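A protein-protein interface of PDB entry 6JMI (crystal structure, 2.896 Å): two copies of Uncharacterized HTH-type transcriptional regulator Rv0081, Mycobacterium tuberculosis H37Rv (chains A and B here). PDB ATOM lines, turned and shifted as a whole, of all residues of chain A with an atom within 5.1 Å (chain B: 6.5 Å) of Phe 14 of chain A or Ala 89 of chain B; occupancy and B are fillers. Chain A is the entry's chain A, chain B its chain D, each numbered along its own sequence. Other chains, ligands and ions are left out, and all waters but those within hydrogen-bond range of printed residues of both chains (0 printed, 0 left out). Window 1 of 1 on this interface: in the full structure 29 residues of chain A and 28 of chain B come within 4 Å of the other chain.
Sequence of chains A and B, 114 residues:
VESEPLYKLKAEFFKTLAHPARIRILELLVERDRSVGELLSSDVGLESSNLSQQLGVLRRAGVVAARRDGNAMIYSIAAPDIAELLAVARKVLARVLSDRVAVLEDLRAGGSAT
O of Phe 13 of chain A sits at hydrogen-bond distance from OG1 of Thr 16 of chain A, 2.5 Å away.
Among the printed residues, merely in contact across the chains: Lys 10 of chain A with Ile 23 of chain B (3.6 Å), Lys 10 of chain A with Leu 93 of chain B (3.6 Å), Ala 11 of chain A with Ala 18 of chain B (3.4 Å), Ala 11 of chain A with His 19 of chain B (3.6 Å), Ala 11 of chain A with Ile 23 of chain B (3.6 Å), Phe 13 of chain A with Val 92 of chain B (3.6 Å), Phe 13 of chain A with Leu 93 of chain B (3.95 Å), Phe 14 of chain A with Phe 14 of chain B (3.5 Å), Phe 14 of chain A with Leu 17 of chain B (3.3 Å), Phe 14 of chain A with Ala 18 of chain B (3.9999 Å), Phe 14 of chain A with Ala 89 of chain B (3.6 Å), Lys 15 of chain A with Ala 18 of chain B (3.6 Å), Leu 17 of chain A with Phe 14 of chain B (3.2 Å), Ala 18 of chain A with Ala 11 of chain B (3.5 Å), Ala 18 of chain A with Lys 15 of chain B (3.6 Å) and Leu 85 of chain A with Val 88 of chain B (3.7 Å).
Of the printed residues of chain B, Phe 14 of chain A touches Phe 14, Leu 17, Ala 18 and Ala 89. Ala 89 of chain B touches just one residue of chain A: Phe 14 (3.6 Å). Of the printed residues of chain B, Ala 11 of chain A touches Ala 18 (3.4 Å), His 19 (3.6 Å) and Ile 23 (3.6 Å). Printed residues of chain A within 4 Å of Val 92 of chain B: Phe 13 (3.6 Å). Printed residues of chain B within 4 Å of Ala 18 of chain A: Ala 11 and Lys 15. Glu 12 of chain A touches none of the printed residues of chain B. Ala 94 of chain B touches none of the printed residues of chain A. The nearest printed residue of chain B that does not touch Phe 14 of chain A is Ile 23 of chain B (4.2 Å). The nearest residue of chain A that does not touch Ala 89 of chain B is Leu 85 of chain A (4.1 Å). The nearest printed residue of chain A that does not touch His 19 of chain B is Phe 14 of chain A (6.1 Å).
Hydrophobic or aromatic side chains of chain B within 4 Å of the printed part of chain A: Ala 11, Phe 14, Leu 17, Ala 18, Ile 23, Val 88, Ala 89, Val 92 and Leu 93. Hydrophobic or aromatic side chains of chain A within 4 Å of the printed part of chain B: Ala 11, Phe 13, Phe 14, Leu 17, Ala 18 and Leu 85. Among the printed residues, 16 pairs touch across the chains. Among the printed residues, no Asp or Glu carboxylate lies within 4 Å of a Lys or Arg side-chain nitrogen of the other chain.
Phe 14 of chain B touches its own counterpart, Phe 14 of chain A. Phe 14 of chain A touches Leu 17 of chain B, and with the chains exchanged Leu 17 of chain A touches Phe 14 of chain B. Phe 14 of chain A touches Ala 18 of chain B, but with the chains exchanged Ala 18 of chain A does not touch Phe 14 of chain B (4.01 Å). Lys 15 of chain A touches Ala 18 of chain B, and with the chains exchanged Ala 18 of chain A touches Lys 15 of chain B.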
ATOM      1  N   LYS A  10      -4.935 -12.254 -10.369  1.00  0.00           N
ATOM      2  CA  LYS A  10      -4.444 -12.683 -11.674  1.00  0.00           C
ATOM      3  C   LYS A  10      -3.005 -12.234 -11.891  1.00  0.00           C
ATOM      4  O   LYS A  10      -2.198 -12.975 -12.464  1.00  0.00           O
ATOM      5  CB  LYS A  10      -5.349 -12.147 -12.784  1.00  0.00           C
ATOM      6  CG  LYS A  10      -6.796 -12.601 -12.687  1.00  0.00           C
ATOM      7  CD  LYS A  10      -7.611 -12.089 -13.863  1.00  0.00           C
ATOM      8  CE  LYS A  10      -9.041 -12.599 -13.811  1.00  0.00           C
ATOM      9  NZ  LYS A  10      -9.885 -11.988 -14.876  1.00  0.00           N
ATOM     10  N   ALA A  11      -2.668 -11.025 -11.441  1.00  0.00           N
ATOM     11  CA  ALA A  11      -1.293 -10.550 -11.561  1.00  0.00           C
ATOM     12  C   ALA A  11      -0.375 -11.285 -10.594  1.00  0.00           C
ATOM     13  O   ALA A  11       0.764 -11.618 -10.942  1.00  0.00           O
ATOM     14  CB  ALA A  11      -1.233  -9.043 -11.320  1.00  0.00           C
ATOM     15  N   GLU A  12      -0.852 -11.543  -9.374  1.00  0.00           N
ATOM     16  CA  GLU A  12      -0.050 -12.288  -8.409  1.00  0.00           C
ATOM     17  C   GLU A  12       0.154 -13.731  -8.848  1.00  0.00           C
ATOM     18  O   GLU A  12       1.142 -14.362  -8.457  1.00  0.00           O
ATOM     19  CB  GLU A  12      -0.708 -12.240  -7.029  1.00  0.00           C
ATOM     20  N   PHE A  13      -0.765 -14.269  -9.654  1.00  0.00           N
ATOM     21  CA  PHE A  13      -0.591 -15.622 -10.173  1.00  0.00           C
ATOM     22  C   PHE A  13       0.579 -15.688 -11.145  1.00  0.00           C
ATOM     23  O   PHE A  13       1.423 -16.586 -11.055  1.00  0.00           O
ATOM     24  CB  PHE A  13      -1.880 -16.099 -10.843  1.00  0.00           C
ATOM     25  CG  PHE A  13      -1.771 -17.465 -11.458  1.00  0.00           C
ATOM     26  CD1 PHE A  13      -1.827 -18.602 -10.669  1.00  0.00           C
ATOM     27  CD2 PHE A  13      -1.616 -17.614 -12.827  1.00  0.00           C
ATOM     28  CE1 PHE A  13      -1.727 -19.861 -11.232  1.00  0.00           C
ATOM     29  CE2 PHE A  13      -1.517 -18.870 -13.396  1.00  0.00           C
ATOM     30  CZ  PHE A  13      -1.572 -19.994 -12.597  1.00  0.00           C
ATOM     31  N   PHE A  14       0.653 -14.736 -12.079  1.00  0.00           N
ATOM     32  CA  PHE A  14       1.771 -14.714 -13.016  1.00  0.00           C
ATOM     33  C   PHE A  14       3.068 -14.295 -12.339  1.00  0.00           C
ATOM     34  O   PHE A  14       4.150 -14.705 -12.773  1.00  0.00           O
ATOM     35  CB  PHE A  14       1.459 -13.780 -14.186  1.00  0.00           C
ATOM     36  CG  PHE A  14       0.448 -14.330 -15.150  1.00  0.00           C
ATOM     37  CD1 PHE A  14       0.374 -15.691 -15.393  1.00  0.00           C
ATOM     38  CD2 PHE A  14      -0.428 -13.487 -15.814  1.00  0.00           C
ATOM     39  CE1 PHE A  14      -0.554 -16.202 -16.282  1.00  0.00           C
ATOM     40  CE2 PHE A  14      -1.359 -13.992 -16.702  1.00  0.00           C
ATOM     41  CZ  PHE A  14      -1.422 -15.351 -16.937  1.00  0.00           C
ATOM     42  N   LYS A  15       2.986 -13.481 -11.283  1.00  0.00           N
ATOM     43  CA  LYS A  15       4.188 -13.108 -10.544  1.00  0.00           C
ATOM     44  C   LYS A  15       4.812 -14.309  -9.844  1.00  0.00           C
ATOM     45  O   LYS A  15       6.034 -14.353  -9.664  1.00  0.00           O
ATOM     46  CB  LYS A  15       3.863 -12.009  -9.532  1.00  0.00           C
ATOM     47  CG  LYS A  15       5.076 -11.458  -8.797  1.00  0.00           C
ATOM     48  CD  LYS A  15       4.676 -10.418  -7.765  1.00  0.00           C
ATOM     49  N   THR A  16       3.996 -15.291  -9.451  1.00  0.00           N
ATOM     50  CA  THR A  16       4.533 -16.485  -8.806  1.00  0.00           C
ATOM     51  C   THR A  16       5.365 -17.321  -9.770  1.00  0.00           C
ATOM     52  O   THR A  16       6.287 -18.022  -9.340  1.00  0.00           O
ATOM     53  CB  THR A  16       3.397 -17.326  -8.224  1.00  0.00           C
ATOM     54  OG1 THR A  16       2.138 -16.775  -8.626  1.00  0.00           O
ATOM     55  CG2 THR A  16       3.474 -17.345  -6.705  1.00  0.00           C
ATOM     56  N   LEU A  17       5.061 -17.263 -11.063  1.00  0.00           N
ATOM     57  CA  LEU A  17       5.805 -18.003 -12.073  1.00  0.00           C
ATOM     58  C   LEU A  17       6.948 -17.197 -12.675  1.00  0.00           C
ATOM     59  O   LEU A  17       7.691 -17.729 -13.504  1.00  0.00           O
ATOM     60  CB  LEU A  17       4.871 -18.484 -13.192  1.00  0.00           C
ATOM     61  CG  LEU A  17       3.867 -19.619 -12.948  1.00  0.00           C
ATOM     62  CD1 LEU A  17       2.791 -19.270 -11.933  1.00  0.00           C
ATOM     63  CD2 LEU A  17       3.231 -20.044 -14.266  1.00  0.00           C
ATOM     64  N   ALA A  18       7.109 -15.938 -12.284  1.00  0.00           N
ATOM     65  CA  ALA A  18       8.147 -15.073 -12.844  1.00  0.00           C
ATOM     66  C   ALA A  18       9.459 -15.196 -12.074  1.00  0.00           C
ATOM     67  O   ALA A  18      10.048 -14.206 -11.642  1.00  0.00           O
ATOM     68  CB  ALA A  18       7.662 -13.629 -12.871  1.00  0.00           C
ATOM     69  N   LEU A  85      -0.602 -25.192 -19.272  1.00  0.00           N
ATOM     70  CA  LEU A  85      -0.291 -23.771 -19.156  1.00  0.00           C
ATOM     71  C   LEU A  85       1.143 -23.489 -19.588  1.00  0.00           C
ATOM     72  O   LEU A  85       1.398 -22.552 -20.355  1.00  0.00           O
ATOM     73  CB  LEU A  85      -0.526 -23.300 -17.720  1.00  0.00           C
ATOM     74  CG  LEU A  85      -0.130 -21.858 -17.387  1.00  0.00           C
ATOM     75  CD1 LEU A  85      -0.927 -20.866 -18.215  1.00  0.00           C
ATOM     76  CD2 LEU A  85      -0.308 -21.582 -15.902  1.00  0.00           C
ATOM     77  N   ALA B  11      11.269 -15.941 -17.223  1.00  0.00           N
ATOM     78  CA  ALA B  11      10.705 -15.217 -16.090  1.00  0.00           C
ATOM     79  C   ALA B  11      10.193 -13.846 -16.512  1.00  0.00           C
ATOM     80  O   ALA B  11       9.169 -13.375 -16.002  1.00  0.00           O
ATOM     81  CB  ALA B  11      11.746 -15.086 -14.979  1.00  0.00           C
ATOM     82  N   PHE B  14       6.522 -14.002 -17.915  1.00  0.00           N
ATOM     83  CA  PHE B  14       5.466 -13.968 -16.910  1.00  0.00           C
ATOM     84  C   PHE B  14       5.471 -12.664 -16.125  1.00  0.00           C
ATOM     85  O   PHE B  14       4.407 -12.192 -15.708  1.00  0.00           O
ATOM     86  CB  PHE B  14       5.609 -15.153 -15.955  1.00  0.00           C
ATOM     87  CG  PHE B  14       5.389 -16.488 -16.606  1.00  0.00           C
ATOM     88  CD1 PHE B  14       4.353 -16.675 -17.505  1.00  0.00           C
ATOM     89  CD2 PHE B  14       6.225 -17.556 -16.324  1.00  0.00           C
ATOM     90  CE1 PHE B  14       4.150 -17.903 -18.106  1.00  0.00           C
ATOM     91  CE2 PHE B  14       6.027 -18.786 -16.921  1.00  0.00           C
ATOM     92  CZ  PHE B  14       4.989 -18.959 -17.813  1.00  0.00           C
ATOM     93  N   LYS B  15       6.650 -12.071 -15.914  1.00  0.00           N
ATOM     94  CA  LYS B  15       6.731 -10.819 -15.170  1.00  0.00           C
ATOM     95  C   LYS B  15       6.056  -9.678 -15.918  1.00  0.00           C
ATOM     96  O   LYS B  15       5.509  -8.765 -15.291  1.00  0.00           O
ATOM     97  CB  LYS B  15       8.193 -10.479 -14.880  1.00  0.00           C
ATOM     98  CG  LYS B  15       8.391  -9.381 -13.849  1.00  0.00           C
ATOM     99  CD  LYS B  15       9.864  -9.199 -13.522  1.00  0.00           C
ATOM    100  CE  LYS B  15      10.063  -8.210 -12.384  1.00  0.00           C
ATOM    101  NZ  LYS B  15       9.551  -6.856 -12.725  1.00  0.00           N
ATOM    102  N   LEU B  17       3.353 -10.015 -17.801  1.00  0.00           N
ATOM    103  CA  LEU B  17       1.921 -10.230 -17.635  1.00  0.00           C
ATOM    104  C   LEU B  17       1.463 -10.122 -16.186  1.00  0.00           C
ATOM    105  O   LEU B  17       0.267 -10.275 -15.921  1.00  0.00           O
ATOM    106  CB  LEU B  17       1.524 -11.601 -18.194  1.00  0.00           C
ATOM    107  CG  LEU B  17       1.254 -11.726 -19.697  1.00  0.00           C
ATOM    108  CD1 LEU B  17       2.520 -11.532 -20.521  1.00  0.00           C
ATOM    109  CD2 LEU B  17       0.612 -13.070 -20.010  1.00  0.00           C
ATOM    110  N   ALA B  18       2.373  -9.862 -15.249  1.00  0.00           N
ATOM    111  CA  ALA B  18       2.025  -9.779 -13.830  1.00  0.00           C
ATOM    112  C   ALA B  18       1.700  -8.335 -13.438  1.00  0.00           C
ATOM    113  O   ALA B  18       2.320  -7.736 -12.560  1.00  0.00           O
ATOM    114  CB  ALA B  18       3.151 -10.347 -12.976  1.00  0.00           C
ATOM    115  N   HIS B  19       0.695  -7.778 -14.119  1.00  0.00           N
ATOM    116  CA  HIS B  19       0.242  -6.421 -13.861  1.00  0.00           C
ATOM    117  C   HIS B  19      -1.261  -6.362 -14.094  1.00  0.00           C
ATOM    118  O   HIS B  19      -1.720  -6.742 -15.184  1.00  0.00           O
ATOM    119  CB  HIS B  19       0.950  -5.399 -14.751  1.00  0.00           C
ATOM    120  CG  HIS B  19       2.417  -5.279 -14.486  1.00  0.00           C
ATOM    121  ND1 HIS B  19       2.925  -4.549 -13.433  1.00  0.00           N
ATOM    122  CD2 HIS B  19       3.487  -5.797 -15.135  1.00  0.00           C
ATOM    123  CE1 HIS B  19       4.244  -4.623 -13.444  1.00  0.00           C
ATOM    124  NE2 HIS B  19       4.611  -5.374 -14.468  1.00  0.00           N
ATOM    125  N   ILE B  23      -3.158  -6.892 -17.748  1.00  0.00           N
ATOM    126  CA  ILE B  23      -4.049  -8.031 -17.946  1.00  0.00           C
ATOM    127  C   ILE B  23      -5.383  -7.572 -18.520  1.00  0.00           C
ATOM    128  O   ILE B  23      -5.939  -8.211 -19.422  1.00  0.00           O
ATOM    129  CB  ILE B  23      -4.230  -8.803 -16.626  1.00  0.00           C
ATOM    130  CG1 ILE B  23      -2.925  -9.498 -16.233  1.00  0.00           C
ATOM    131  CG2 ILE B  23      -5.356  -9.818 -16.744  1.00  0.00           C
ATOM    132  CD1 ILE B  23      -3.011 -10.275 -14.939  1.00  0.00           C
ATOM    133  N   GLU B  84      -5.468 -18.434 -26.371  1.00  0.00           N
ATOM    134  CA  GLU B  84      -5.462 -19.672 -25.604  1.00  0.00           C
ATOM    135  C   GLU B  84      -4.543 -19.595 -24.392  1.00  0.00           C
ATOM    136  O   GLU B  84      -4.687 -20.405 -23.471  1.00  0.00           O
ATOM    137  CB  GLU B  84      -5.062 -20.851 -26.495  1.00  0.00           C
ATOM    138  CG  GLU B  84      -3.765 -20.657 -27.260  1.00  0.00           C
ATOM    139  CD  GLU B  84      -3.383 -21.884 -28.065  1.00  0.00           C
ATOM    140  OE1 GLU B  84      -3.813 -22.998 -27.693  1.00  0.00           O
ATOM    141  OE2 GLU B  84      -2.656 -21.738 -29.071  1.00  0.00           O
ATOM    142  N   LEU B  85      -3.608 -18.643 -24.369  1.00  0.00           N
ATOM    143  CA  LEU B  85      -2.785 -18.447 -23.180  1.00  0.00           C
ATOM    144  C   LEU B  85      -3.619 -17.898 -22.029  1.00  0.00           C
ATOM    145  O   LEU B  85      -3.558 -18.408 -20.905  1.00  0.00           O
ATOM    146  CB  LEU B  85      -1.616 -17.513 -23.492  1.00  0.00           C
ATOM    147  CG  LEU B  85      -0.759 -17.100 -22.292  1.00  0.00           C
ATOM    148  CD1 LEU B  85      -0.106 -18.313 -21.646  1.00  0.00           C
ATOM    149  CD2 LEU B  85       0.288 -16.073 -22.697  1.00  0.00           C
ATOM    150  N   LEU B  86      -4.406 -16.852 -22.293  1.00  0.00           N
ATOM    151  CA  LEU B  86      -5.302 -16.326 -21.268  1.00  0.00           C
ATOM    152  C   LEU B  86      -6.438 -17.295 -20.970  1.00  0.00           C
ATOM    153  O   LEU B  86      -6.990 -17.279 -19.864  1.00  0.00           O
ATOM    154  CB  LEU B  86      -5.860 -14.971 -21.700  1.00  0.00           C
ATOM    155  CG  LEU B  86      -4.847 -13.840 -21.893  1.00  0.00           C
ATOM    156  CD1 LEU B  86      -5.546 -12.572 -22.355  1.00  0.00           C
ATOM    157  CD2 LEU B  86      -4.070 -13.589 -20.611  1.00  0.00           C
ATOM    158  N   ALA B  87      -6.800 -18.139 -21.937  1.00  0.00           N
ATOM    159  CA  ALA B  87      -7.864 -19.111 -21.711  1.00  0.00           C
ATOM    160  C   ALA B  87      -7.424 -20.185 -20.723  1.00  0.00           C
ATOM    161  O   ALA B  87      -8.162 -20.523 -19.790  1.00  0.00           O
ATOM    162  CB  ALA B  87      -8.293 -19.738 -23.038  1.00  0.00           C
ATOM    163  N   VAL B  88      -6.223 -20.733 -20.912  1.00  0.00           N
ATOM    164  CA  VAL B  88      -5.731 -21.749 -19.988  1.00  0.00           C
ATOM    165  C   VAL B  88      -5.303 -21.120 -18.666  1.00  0.00           C
ATOM    166  O   VAL B  88      -5.329 -21.782 -17.623  1.00  0.00           O
ATOM    167  CB  VAL B  88      -4.589 -22.555 -20.637  1.00  0.00           C
ATOM    168  CG1 VAL B  88      -3.352 -21.690 -20.826  1.00  0.00           C
ATOM    169  CG2 VAL B  88      -4.264 -23.795 -19.810  1.00  0.00           C
ATOM    170  N   ALA B  89      -4.917 -19.841 -18.676  1.00  0.00           N
ATOM    171  CA  ALA B  89      -4.564 -19.174 -17.427  1.00  0.00           C
ATOM    172  C   ALA B  89      -5.789 -18.979 -16.544  1.00  0.00           C
ATOM    173  O   ALA B  89      -5.729 -19.204 -15.330  1.00  0.00           O
ATOM    174  CB  ALA B  89      -3.889 -17.834 -17.717  1.00  0.00           C
ATOM    175  N   ARG B  90      -6.912 -18.565 -17.137  1.00  0.00           N
ATOM    176  CA  ARG B  90      -8.144 -18.429 -16.368  1.00  0.00           C
ATOM    177  C   ARG B  90      -8.680 -19.785 -15.929  1.00  0.00           C
ATOM    178  O   ARG B  90      -9.250 -19.899 -14.838  1.00  0.00           O
ATOM    179  CB  ARG B  90      -9.197 -17.681 -17.185  1.00  0.00           C
ATOM    180  CG  ARG B  90      -8.867 -16.217 -17.430  1.00  0.00           C
ATOM    181  CD  ARG B  90      -9.940 -15.524 -18.257  1.00  0.00           C
ATOM    182  NE  ARG B  90     -10.018 -16.048 -19.618  1.00  0.00           N
ATOM    183  CZ  ARG B  90     -10.934 -16.914 -20.037  1.00  0.00           C
ATOM    184  NH1 ARG B  90     -11.862 -17.360 -19.200  1.00  0.00           N
ATOM    185  NH2 ARG B  90     -10.926 -17.335 -21.295  1.00  0.00           N
ATOM    186  N   LYS B  91      -8.509 -20.820 -16.756  1.00  0.00           N
ATOM    187  CA  LYS B  91      -8.942 -22.157 -16.364  1.00  0.00           C
ATOM    188  C   LYS B  91      -8.135 -22.672 -15.179  1.00  0.00           C
ATOM    189  O   LYS B  91      -8.696 -23.255 -14.244  1.00  0.00           O
ATOM    190  CB  LYS B  91      -8.825 -23.118 -17.547  1.00  0.00           C
ATOM    191  CG  LYS B  91      -9.141 -24.563 -17.195  1.00  0.00           C
ATOM    192  CD  LYS B  91      -8.766 -25.511 -18.321  1.00  0.00           C
ATOM    193  CE  LYS B  91      -8.984 -26.958 -17.911  1.00  0.00           C
ATOM    194  NZ  LYS B  91      -8.567 -27.909 -18.977  1.00  0.00           N
ATOM    195  N   VAL B  92      -6.817 -22.465 -15.200  1.00  0.00           N
ATOM    196  CA  VAL B  92      -5.975 -22.902 -14.091  1.00  0.00           C
ATOM    197  C   VAL B  92      -6.297 -22.108 -12.832  1.00  0.00           C
ATOM    198  O   VAL B  92      -6.434 -22.673 -11.740  1.00  0.00           O
ATOM    199  CB  VAL B  92      -4.487 -22.782 -14.469  1.00  0.00           C
ATOM    200  CG1 VAL B  92      -3.616 -22.871 -13.228  1.00  0.00           C
ATOM    201  CG2 VAL B  92      -4.104 -23.862 -15.467  1.00  0.00           C
ATOM    202  N   LEU B  93      -6.429 -20.787 -12.966  1.00  0.00           N
ATOM    203  CA  LEU B  93      -6.689 -19.948 -11.802  1.00  0.00           C
ATOM    204  C   LEU B  93      -8.059 -20.239 -11.200  1.00  0.00           C
ATOM    205  O   LEU B  93      -8.224 -20.200  -9.974  1.00  0.00           O
ATOM    206  CB  LEU B  93      -6.571 -18.472 -12.183  1.00  0.00           C
ATOM    207  CG  LEU B  93      -6.686 -17.472 -11.031  1.00  0.00           C
ATOM    208  CD1 LEU B  93      -5.624 -17.749  -9.979  1.00  0.00           C
ATOM    209  CD2 LEU B  93      -6.575 -16.050 -11.547  1.00  0.00           C
ATOM    210  N   ALA B  94      -9.052 -20.537 -12.042  1.00  0.00           N
ATOM    211  CA  ALA B  94     -10.377 -20.871 -11.529  1.00  0.00           C
ATOM    212  C   ALA B  94     -10.343 -22.155 -10.713  1.00  0.00           C
ATOM    213  O   ALA B  94     -11.056 -22.283  -9.710  1.00  0.00           O
ATOM    214  CB  ALA B  94     -11.373 -20.991 -12.680  1.00  0.00           C
